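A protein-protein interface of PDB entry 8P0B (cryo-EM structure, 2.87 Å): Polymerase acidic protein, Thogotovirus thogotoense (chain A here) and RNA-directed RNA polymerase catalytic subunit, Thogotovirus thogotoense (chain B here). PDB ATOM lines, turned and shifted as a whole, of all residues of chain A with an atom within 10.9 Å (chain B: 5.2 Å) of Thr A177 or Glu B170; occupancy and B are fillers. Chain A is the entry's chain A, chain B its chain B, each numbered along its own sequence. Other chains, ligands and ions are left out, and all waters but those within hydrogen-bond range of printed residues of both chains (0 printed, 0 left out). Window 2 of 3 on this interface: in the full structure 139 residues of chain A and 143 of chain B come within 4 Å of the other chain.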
ATOM      1  N   PHE A 173       7.334 -20.572  -7.274  1.00  0.00           N
ATOM      2  CA  PHE A 173       8.401 -20.130  -6.388  1.00  0.00           C
ATOM      3  C   PHE A 173       7.938 -18.917  -5.599  1.00  0.00           C
ATOM      4  O   PHE A 173       7.218 -18.061  -6.122  1.00  0.00           O
ATOM      5  CB  PHE A 173       9.676 -19.781  -7.162  1.00  0.00           C
ATOM      6  CG  PHE A 173      10.852 -19.489  -6.278  1.00  0.00           C
ATOM      7  CD1 PHE A 173      11.416 -20.485  -5.501  1.00  0.00           C
ATOM      8  CD2 PHE A 173      11.382 -18.213  -6.212  1.00  0.00           C
ATOM      9  CE1 PHE A 173      12.495 -20.215  -4.683  1.00  0.00           C
ATOM     10  CE2 PHE A 173      12.457 -17.940  -5.394  1.00  0.00           C
ATOM     11  CZ  PHE A 173      13.014 -18.940  -4.629  1.00  0.00           C
ATOM     12  N   SER A 174       8.356 -18.853  -4.339  1.00  0.00           N
ATOM     13  CA  SER A 174       8.072 -17.712  -3.483  1.00  0.00           C
ATOM     14  C   SER A 174       9.202 -17.583  -2.475  1.00  0.00           C
ATOM     15  O   SER A 174       9.758 -18.589  -2.026  1.00  0.00           O
ATOM     16  CB  SER A 174       6.727 -17.866  -2.765  1.00  0.00           C
ATOM     17  OG  SER A 174       6.886 -18.493  -1.505  1.00  0.00           O
ATOM     18  N   VAL A 175       9.536 -16.344  -2.125  1.00  0.00           N
ATOM     19  CA  VAL A 175      10.639 -16.042  -1.220  1.00  0.00           C
ATOM     20  C   VAL A 175      10.057 -15.467   0.064  1.00  0.00           C
ATOM     21  O   VAL A 175       9.191 -14.585   0.023  1.00  0.00           O
ATOM     22  CB  VAL A 175      11.643 -15.069  -1.863  1.00  0.00           C
ATOM     23  CG1 VAL A 175      11.040 -13.681  -1.998  1.00  0.00           C
ATOM     24  CG2 VAL A 175      12.933 -15.023  -1.060  1.00  0.00           C
ATOM     25  N   GLY A 176      10.528 -15.972   1.201  1.00  0.00           N
ATOM     26  CA  GLY A 176      10.010 -15.547   2.486  1.00  0.00           C
ATOM     27  C   GLY A 176      10.342 -14.108   2.814  1.00  0.00           C
ATOM     28  O   GLY A 176      10.701 -13.328   1.926  1.00  0.00           O
ATOM     29  N   THR A 177      10.225 -13.742   4.089  1.00  0.00           N
ATOM     30  CA  THR A 177      10.501 -12.387   4.548  1.00  0.00           C
ATOM     31  C   THR A 177      11.914 -12.239   5.099  1.00  0.00           C
ATOM     32  O   THR A 177      12.640 -11.324   4.704  1.00  0.00           O
ATOM     33  CB  THR A 177       9.484 -11.978   5.621  1.00  0.00           C
ATOM     34  OG1 THR A 177       8.157 -12.244   5.153  1.00  0.00           O
ATOM     35  CG2 THR A 177       9.616 -10.497   5.944  1.00  0.00           C
ATOM     36  N   THR A 178      12.318 -13.125   6.012  1.00  0.00           N
ATOM     37  CA  THR A 178      13.674 -13.058   6.548  1.00  0.00           C
ATOM     38  C   THR A 178      14.705 -13.337   5.463  1.00  0.00           C
ATOM     39  O   THR A 178      15.786 -12.735   5.454  1.00  0.00           O
ATOM     40  CB  THR A 178      13.832 -14.046   7.702  1.00  0.00           C
ATOM     41  OG1 THR A 178      12.602 -14.139   8.430  1.00  0.00           O
ATOM     42  CG2 THR A 178      14.941 -13.593   8.641  1.00  0.00           C
ATOM     43  N   PHE A 179      14.394 -14.254   4.545  1.00  0.00           N
ATOM     44  CA  PHE A 179      15.311 -14.525   3.445  1.00  0.00           C
ATOM     45  C   PHE A 179      15.501 -13.287   2.580  1.00  0.00           C
ATOM     46  O   PHE A 179      16.604 -13.026   2.090  1.00  0.00           O
ATOM     47  CB  PHE A 179      14.793 -15.698   2.609  1.00  0.00           C
ATOM     48  CG  PHE A 179      15.797 -16.246   1.626  1.00  0.00           C
ATOM     49  CD1 PHE A 179      17.160 -16.111   1.837  1.00  0.00           C
ATOM     50  CD2 PHE A 179      15.368 -16.908   0.488  1.00  0.00           C
ATOM     51  CE1 PHE A 179      18.069 -16.621   0.932  1.00  0.00           C
ATOM     52  CE2 PHE A 179      16.274 -17.417  -0.417  1.00  0.00           C
ATOM     53  CZ  PHE A 179      17.625 -17.274  -0.195  1.00  0.00           C
ATOM     54  N   ARG A 180      14.435 -12.506   2.384  1.00  0.00           N
ATOM     55  CA  ARG A 180      14.572 -11.242   1.669  1.00  0.00           C
ATOM     56  C   ARG A 180      15.498 -10.291   2.417  1.00  0.00           C
ATOM     57  O   ARG A 180      16.312  -9.589   1.802  1.00  0.00           O
ATOM     58  CB  ARG A 180      13.200 -10.600   1.471  1.00  0.00           C
ATOM     59  CG  ARG A 180      12.404 -11.170   0.313  1.00  0.00           C
ATOM     60  CD  ARG A 180      11.107 -10.403   0.116  1.00  0.00           C
ATOM     61  NE  ARG A 180      10.912 -10.006  -1.274  1.00  0.00           N
ATOM     62  CZ  ARG A 180       9.987 -10.500  -2.089  1.00  0.00           C
ATOM     63  NH1 ARG A 180       9.122 -11.416  -1.686  1.00  0.00           N
ATOM     64  NH2 ARG A 180       9.926 -10.058  -3.342  1.00  0.00           N
ATOM     65  N   THR A 181      15.380 -10.246   3.745  1.00  0.00           N
ATOM     66  CA  THR A 181      16.267  -9.400   4.535  1.00  0.00           C
ATOM     67  C   THR A 181      17.719  -9.827   4.366  1.00  0.00           C
ATOM     68  O   THR A 181      18.613  -8.983   4.250  1.00  0.00           O
ATOM     69  CB  THR A 181      15.863  -9.450   6.008  1.00  0.00           C
ATOM     70  OG1 THR A 181      14.528  -8.951   6.156  1.00  0.00           O
ATOM     71  CG2 THR A 181      16.809  -8.614   6.857  1.00  0.00           C
ATOM     72  N   LEU A 182      17.972 -11.137   4.356  1.00  0.00           N
ATOM     73  CA  LEU A 182      19.326 -11.623   4.112  1.00  0.00           C
ATOM     74  C   LEU A 182      19.807 -11.223   2.722  1.00  0.00           C
ATOM     75  O   LEU A 182      20.937 -10.754   2.551  1.00  0.00           O
ATOM     76  CB  LEU A 182      19.374 -13.143   4.270  1.00  0.00           C
ATOM     77  CG  LEU A 182      19.030 -13.720   5.643  1.00  0.00           C
ATOM     78  CD1 LEU A 182      19.191 -15.227   5.619  1.00  0.00           C
ATOM     79  CD2 LEU A 182      19.898 -13.109   6.728  1.00  0.00           C
ATOM     80  N   LEU A 183      18.952 -11.399   1.715  1.00  0.00           N
ATOM     81  CA  LEU A 183      19.358 -11.137   0.340  1.00  0.00           C
ATOM     82  C   LEU A 183      19.656  -9.663   0.107  1.00  0.00           C
ATOM     83  O   LEU A 183      20.554  -9.331  -0.675  1.00  0.00           O
ATOM     84  CB  LEU A 183      18.271 -11.611  -0.624  1.00  0.00           C
ATOM     85  CG  LEU A 183      18.051 -13.121  -0.713  1.00  0.00           C
ATOM     86  CD1 LEU A 183      16.705 -13.421  -1.347  1.00  0.00           C
ATOM     87  CD2 LEU A 183      19.167 -13.783  -1.497  1.00  0.00           C
ATOM     88  N   LYS A 184      18.923  -8.766   0.771  1.00  0.00           N
ATOM     89  CA  LYS A 184      19.058  -7.331   0.549  1.00  0.00           C
ATOM     90  C   LYS A 184      20.108  -6.690   1.448  1.00  0.00           C
ATOM     91  O   LYS A 184      20.005  -5.496   1.758  1.00  0.00           O
ATOM     92  CB  LYS A 184      17.706  -6.644   0.746  1.00  0.00           C
ATOM     93  CG  LYS A 184      16.627  -7.098  -0.224  1.00  0.00           C
ATOM     94  CD  LYS A 184      15.283  -6.455   0.091  1.00  0.00           C
ATOM     95  CE  LYS A 184      15.359  -4.938   0.031  1.00  0.00           C
ATOM     96  NZ  LYS A 184      14.046  -4.317  -0.288  1.00  0.00           N
ATOM     97  N   ARG A 185      21.117  -7.447   1.874  1.00  0.00           N
ATOM     98  CA  ARG A 185      22.115  -6.929   2.801  1.00  0.00           C
ATOM     99  C   ARG A 185      23.290  -6.255   2.107  1.00  0.00           C
ATOM    100  O   ARG A 185      23.893  -5.343   2.683  1.00  0.00           O
ATOM    101  CB  ARG A 185      22.644  -8.058   3.688  1.00  0.00           C
ATOM    102  CG  ARG A 185      22.125  -8.019   5.112  1.00  0.00           C
ATOM    103  CD  ARG A 185      22.688  -9.162   5.939  1.00  0.00           C
ATOM    104  NE  ARG A 185      21.831  -9.490   7.071  1.00  0.00           N
ATOM    105  CZ  ARG A 185      21.866 -10.639   7.732  1.00  0.00           C
ATOM    106  NH1 ARG A 185      22.717 -11.598   7.408  1.00  0.00           N
ATOM    107  NH2 ARG A 185      21.026 -10.829   8.745  1.00  0.00           N
ATOM    108  N   VAL A 191      14.974  -7.328  -4.331  1.00  0.00           N
ATOM    109  CA  VAL A 191      15.066  -8.602  -5.038  1.00  0.00           C
ATOM    110  C   VAL A 191      14.763  -8.405  -6.515  1.00  0.00           C
ATOM    111  O   VAL A 191      15.430  -8.979  -7.384  1.00  0.00           O
ATOM    112  CB  VAL A 191      14.128  -9.641  -4.397  1.00  0.00           C
ATOM    113  CG1 VAL A 191      14.052 -10.892  -5.260  1.00  0.00           C
ATOM    114  CG2 VAL A 191      14.602  -9.984  -2.995  1.00  0.00           C
ATOM    115  N   ALA B 166      14.594 -21.966  -0.327  1.00  0.00           N
ATOM    116  CA  ALA B 166      14.039 -20.685   0.090  1.00  0.00           C
ATOM    117  C   ALA B 166      13.159 -20.822   1.322  1.00  0.00           C
ATOM    118  O   ALA B 166      12.969 -19.841   2.050  1.00  0.00           O
ATOM    119  CB  ALA B 166      13.241 -20.065  -1.055  1.00  0.00           C
ATOM    120  N   ASP B 167      12.616 -22.014   1.566  1.00  0.00           N
ATOM    121  CA  ASP B 167      11.799 -22.238   2.751  1.00  0.00           C
ATOM    122  C   ASP B 167      12.660 -22.535   3.970  1.00  0.00           C
ATOM    123  O   ASP B 167      12.392 -22.024   5.062  1.00  0.00           O
ATOM    124  CB  ASP B 167      10.819 -23.385   2.505  1.00  0.00           C
ATOM    125  CG  ASP B 167       9.413 -23.049   2.952  1.00  0.00           C
ATOM    126  OD1 ASP B 167       9.239 -22.680   4.133  1.00  0.00           O
ATOM    127  OD2 ASP B 167       8.483 -23.149   2.126  1.00  0.00           O
ATOM    128  N   VAL B 168      13.690 -23.370   3.811  1.00  0.00           N
ATOM    129  CA  VAL B 168      14.546 -23.666   4.955  1.00  0.00           C
ATOM    130  C   VAL B 168      15.214 -22.387   5.420  1.00  0.00           C
ATOM    131  O   VAL B 168      15.447 -22.196   6.619  1.00  0.00           O
ATOM    132  CB  VAL B 168      15.607 -24.738   4.630  1.00  0.00           C
ATOM    133  CG1 VAL B 168      16.318 -24.437   3.324  1.00  0.00           C
ATOM    134  CG2 VAL B 168      16.599 -24.869   5.771  1.00  0.00           C
ATOM    135  N   MET B 169      15.531 -21.485   4.486  1.00  0.00           N
ATOM    136  CA  MET B 169      16.178 -20.240   4.875  1.00  0.00           C
ATOM    137  C   MET B 169      15.299 -19.392   5.783  1.00  0.00           C
ATOM    138  O   MET B 169      15.821 -18.548   6.518  1.00  0.00           O
ATOM    139  CB  MET B 169      16.552 -19.431   3.633  1.00  0.00           C
ATOM    140  CG  MET B 169      17.941 -19.701   3.059  1.00  0.00           C
ATOM    141  SD  MET B 169      19.216 -20.268   4.205  1.00  0.00           S
ATOM    142  CE  MET B 169      19.341 -18.854   5.295  1.00  0.00           C
ATOM    143  N   GLU B 170      13.982 -19.595   5.750  1.00  0.00           N
ATOM    144  CA  GLU B 170      13.093 -18.873   6.649  1.00  0.00           C
ATOM    145  C   GLU B 170      13.137 -19.417   8.069  1.00  0.00           C
ATOM    146  O   GLU B 170      12.809 -18.685   9.008  1.00  0.00           O
ATOM    147  CB  GLU B 170      11.659 -18.929   6.121  1.00  0.00           C
ATOM    148  CG  GLU B 170      11.326 -17.834   5.124  1.00  0.00           C
ATOM    149  CD  GLU B 170      11.268 -16.462   5.762  1.00  0.00           C
ATOM    150  OE1 GLU B 170      12.323 -15.800   5.846  1.00  0.00           O
ATOM    151  OE2 GLU B 170      10.169 -16.045   6.181  1.00  0.00           O
ATOM    152  N   LEU B 171      13.532 -20.675   8.246  1.00  0.00           N
ATOM    153  CA  LEU B 171      13.580 -21.260   9.579  1.00  0.00           C
ATOM    154  C   LEU B 171      14.551 -20.491  10.463  1.00  0.00           C
ATOM    155  O   LEU B 171      15.637 -20.097  10.029  1.00  0.00           O
ATOM    156  CB  LEU B 171      13.995 -22.730   9.500  1.00  0.00           C
ATOM    157  CG  LEU B 171      13.050 -23.662   8.740  1.00  0.00           C
ATOM    158  CD1 LEU B 171      13.716 -25.000   8.486  1.00  0.00           C
ATOM    159  CD2 LEU B 171      11.751 -23.851   9.498  1.00  0.00           C
ATOM    160  N   ASP B 172      14.152 -20.278  11.719  1.00  0.00           N
ATOM    161  CA  ASP B 172      15.019 -19.586  12.665  1.00  0.00           C
ATOM    162  C   ASP B 172      16.258 -20.402  13.004  1.00  0.00           C
ATOM    163  O   ASP B 172      17.300 -19.821  13.325  1.00  0.00           O
ATOM    164  CB  ASP B 172      14.253 -19.261  13.948  1.00  0.00           C
ATOM    165  CG  ASP B 172      12.824 -18.831  13.684  1.00  0.00           C
ATOM    166  OD1 ASP B 172      12.026 -19.673  13.223  1.00  0.00           O
ATOM    167  OD2 ASP B 172      12.498 -17.653  13.940  1.00  0.00           O
ATOM    168  N   ARG B 216      20.249 -19.450  11.631  1.00  0.00           N
ATOM    169  CA  ARG B 216      19.915 -18.870  10.336  1.00  0.00           C
ATOM    170  C   ARG B 216      21.110 -18.135   9.747  1.00  0.00           C
ATOM    171  O   ARG B 216      21.399 -18.257   8.551  1.00  0.00           O
ATOM    172  CB  ARG B 216      18.718 -17.926  10.468  1.00  0.00           C
ATOM    173  CG  ARG B 216      18.019 -17.642   9.147  1.00  0.00           C
ATOM    174  CD  ARG B 216      17.377 -16.265   9.136  1.00  0.00           C
ATOM    175  NE  ARG B 216      16.575 -16.022  10.328  1.00  0.00           N
ATOM    176  CZ  ARG B 216      15.371 -16.536  10.542  1.00  0.00           C
ATOM    177  NH1 ARG B 216      14.795 -17.341   9.664  1.00  0.00           N
ATOM    178  NH2 ARG B 216      14.728 -16.233  11.666  1.00  0.00           N
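The backbone NH (N) of Thr A177 is in hydrogen-bond range of the side-chain carboxylate (OE2) of Glu B170 (3.1 Å). The side-chain carboxylate (OE1) of Glu B170 is in hydrogen-bond range of the backbone NH (N) of Thr A178, 2.7 Å away. N of Phe A179 sits at hydrogen-bond distance from OE1 of Glu B170, 2.9 Å away.
Printed residues of chain A that touch a printed residue of chain B: Phe A173, Ser A174, Gly A176, Thr A177, Thr A178, Phe A179 and Leu A182. Of the 8 printed residues of chain B, 4 touch a printed residue of chain A. Hydrophobic or aromatic side chains of chain B within 4 Å of the printed part of chain A: Ala B166 and Met B169.
Printed residues of chain B within 4 Å of Ser A174: Ala B166 (3.9 Å). Of the printed residues of chain B, Gly A176 touches Glu B170. Thr A177 touches just one residue of chain B: Glu B170 (3.1 Å). Of the printed residues of chain B, Thr A178 touches Glu B170 (2.7 Å) and Arg B216 (3.4 Å). Val A191 touches none of the printed residues of chain B. No residue of chain A comes within 4 Å of Asp B167. Met B169 touches just these residues of chain A: Phe A179 (3.7 Å) and Leu A182 (3.6 Å). Glu B170 touches four residues of chain A. Leu B171 touches none of the printed residues of chain A. Asp B172 touches none of the printed residues of chain A. The nearest printed residue of chain B that does not touch Ser A174 is Asp B167 (5.7 Å).
Ala B166 touches Phe A173. Ser A174 touches Ala B166. Glu B170 touches Gly A176. NE of Arg B216 touches CG2 of Thr A178, 3.4 Å away. Phe A179 touches Ala B166 (CE2 to CA, 3.99 Å). Phe A179 touches Met B169 (CE1 to CG, 3.7 Å). Leu A182 touches Met B169 (CD1 to CE, 3.6 Å).
O of Thr A177 sits at hydrogen-bond distance from OG1 of Thr A181 (3.4 Å). The guanidinium group (NH1) of Arg B216 sits at hydrogen-bond distance from the backbone carbonyl oxygen (O) of Glu B170, 2.5 Å away. NH1 of Arg B216 lies within hydrogen-bond range of O of Leu B171 (2.9 Å). The side-chain carboxylate of Asp B172 lies within salt-bridge range of the guanidinium group of Arg B216 (3.5 Å).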
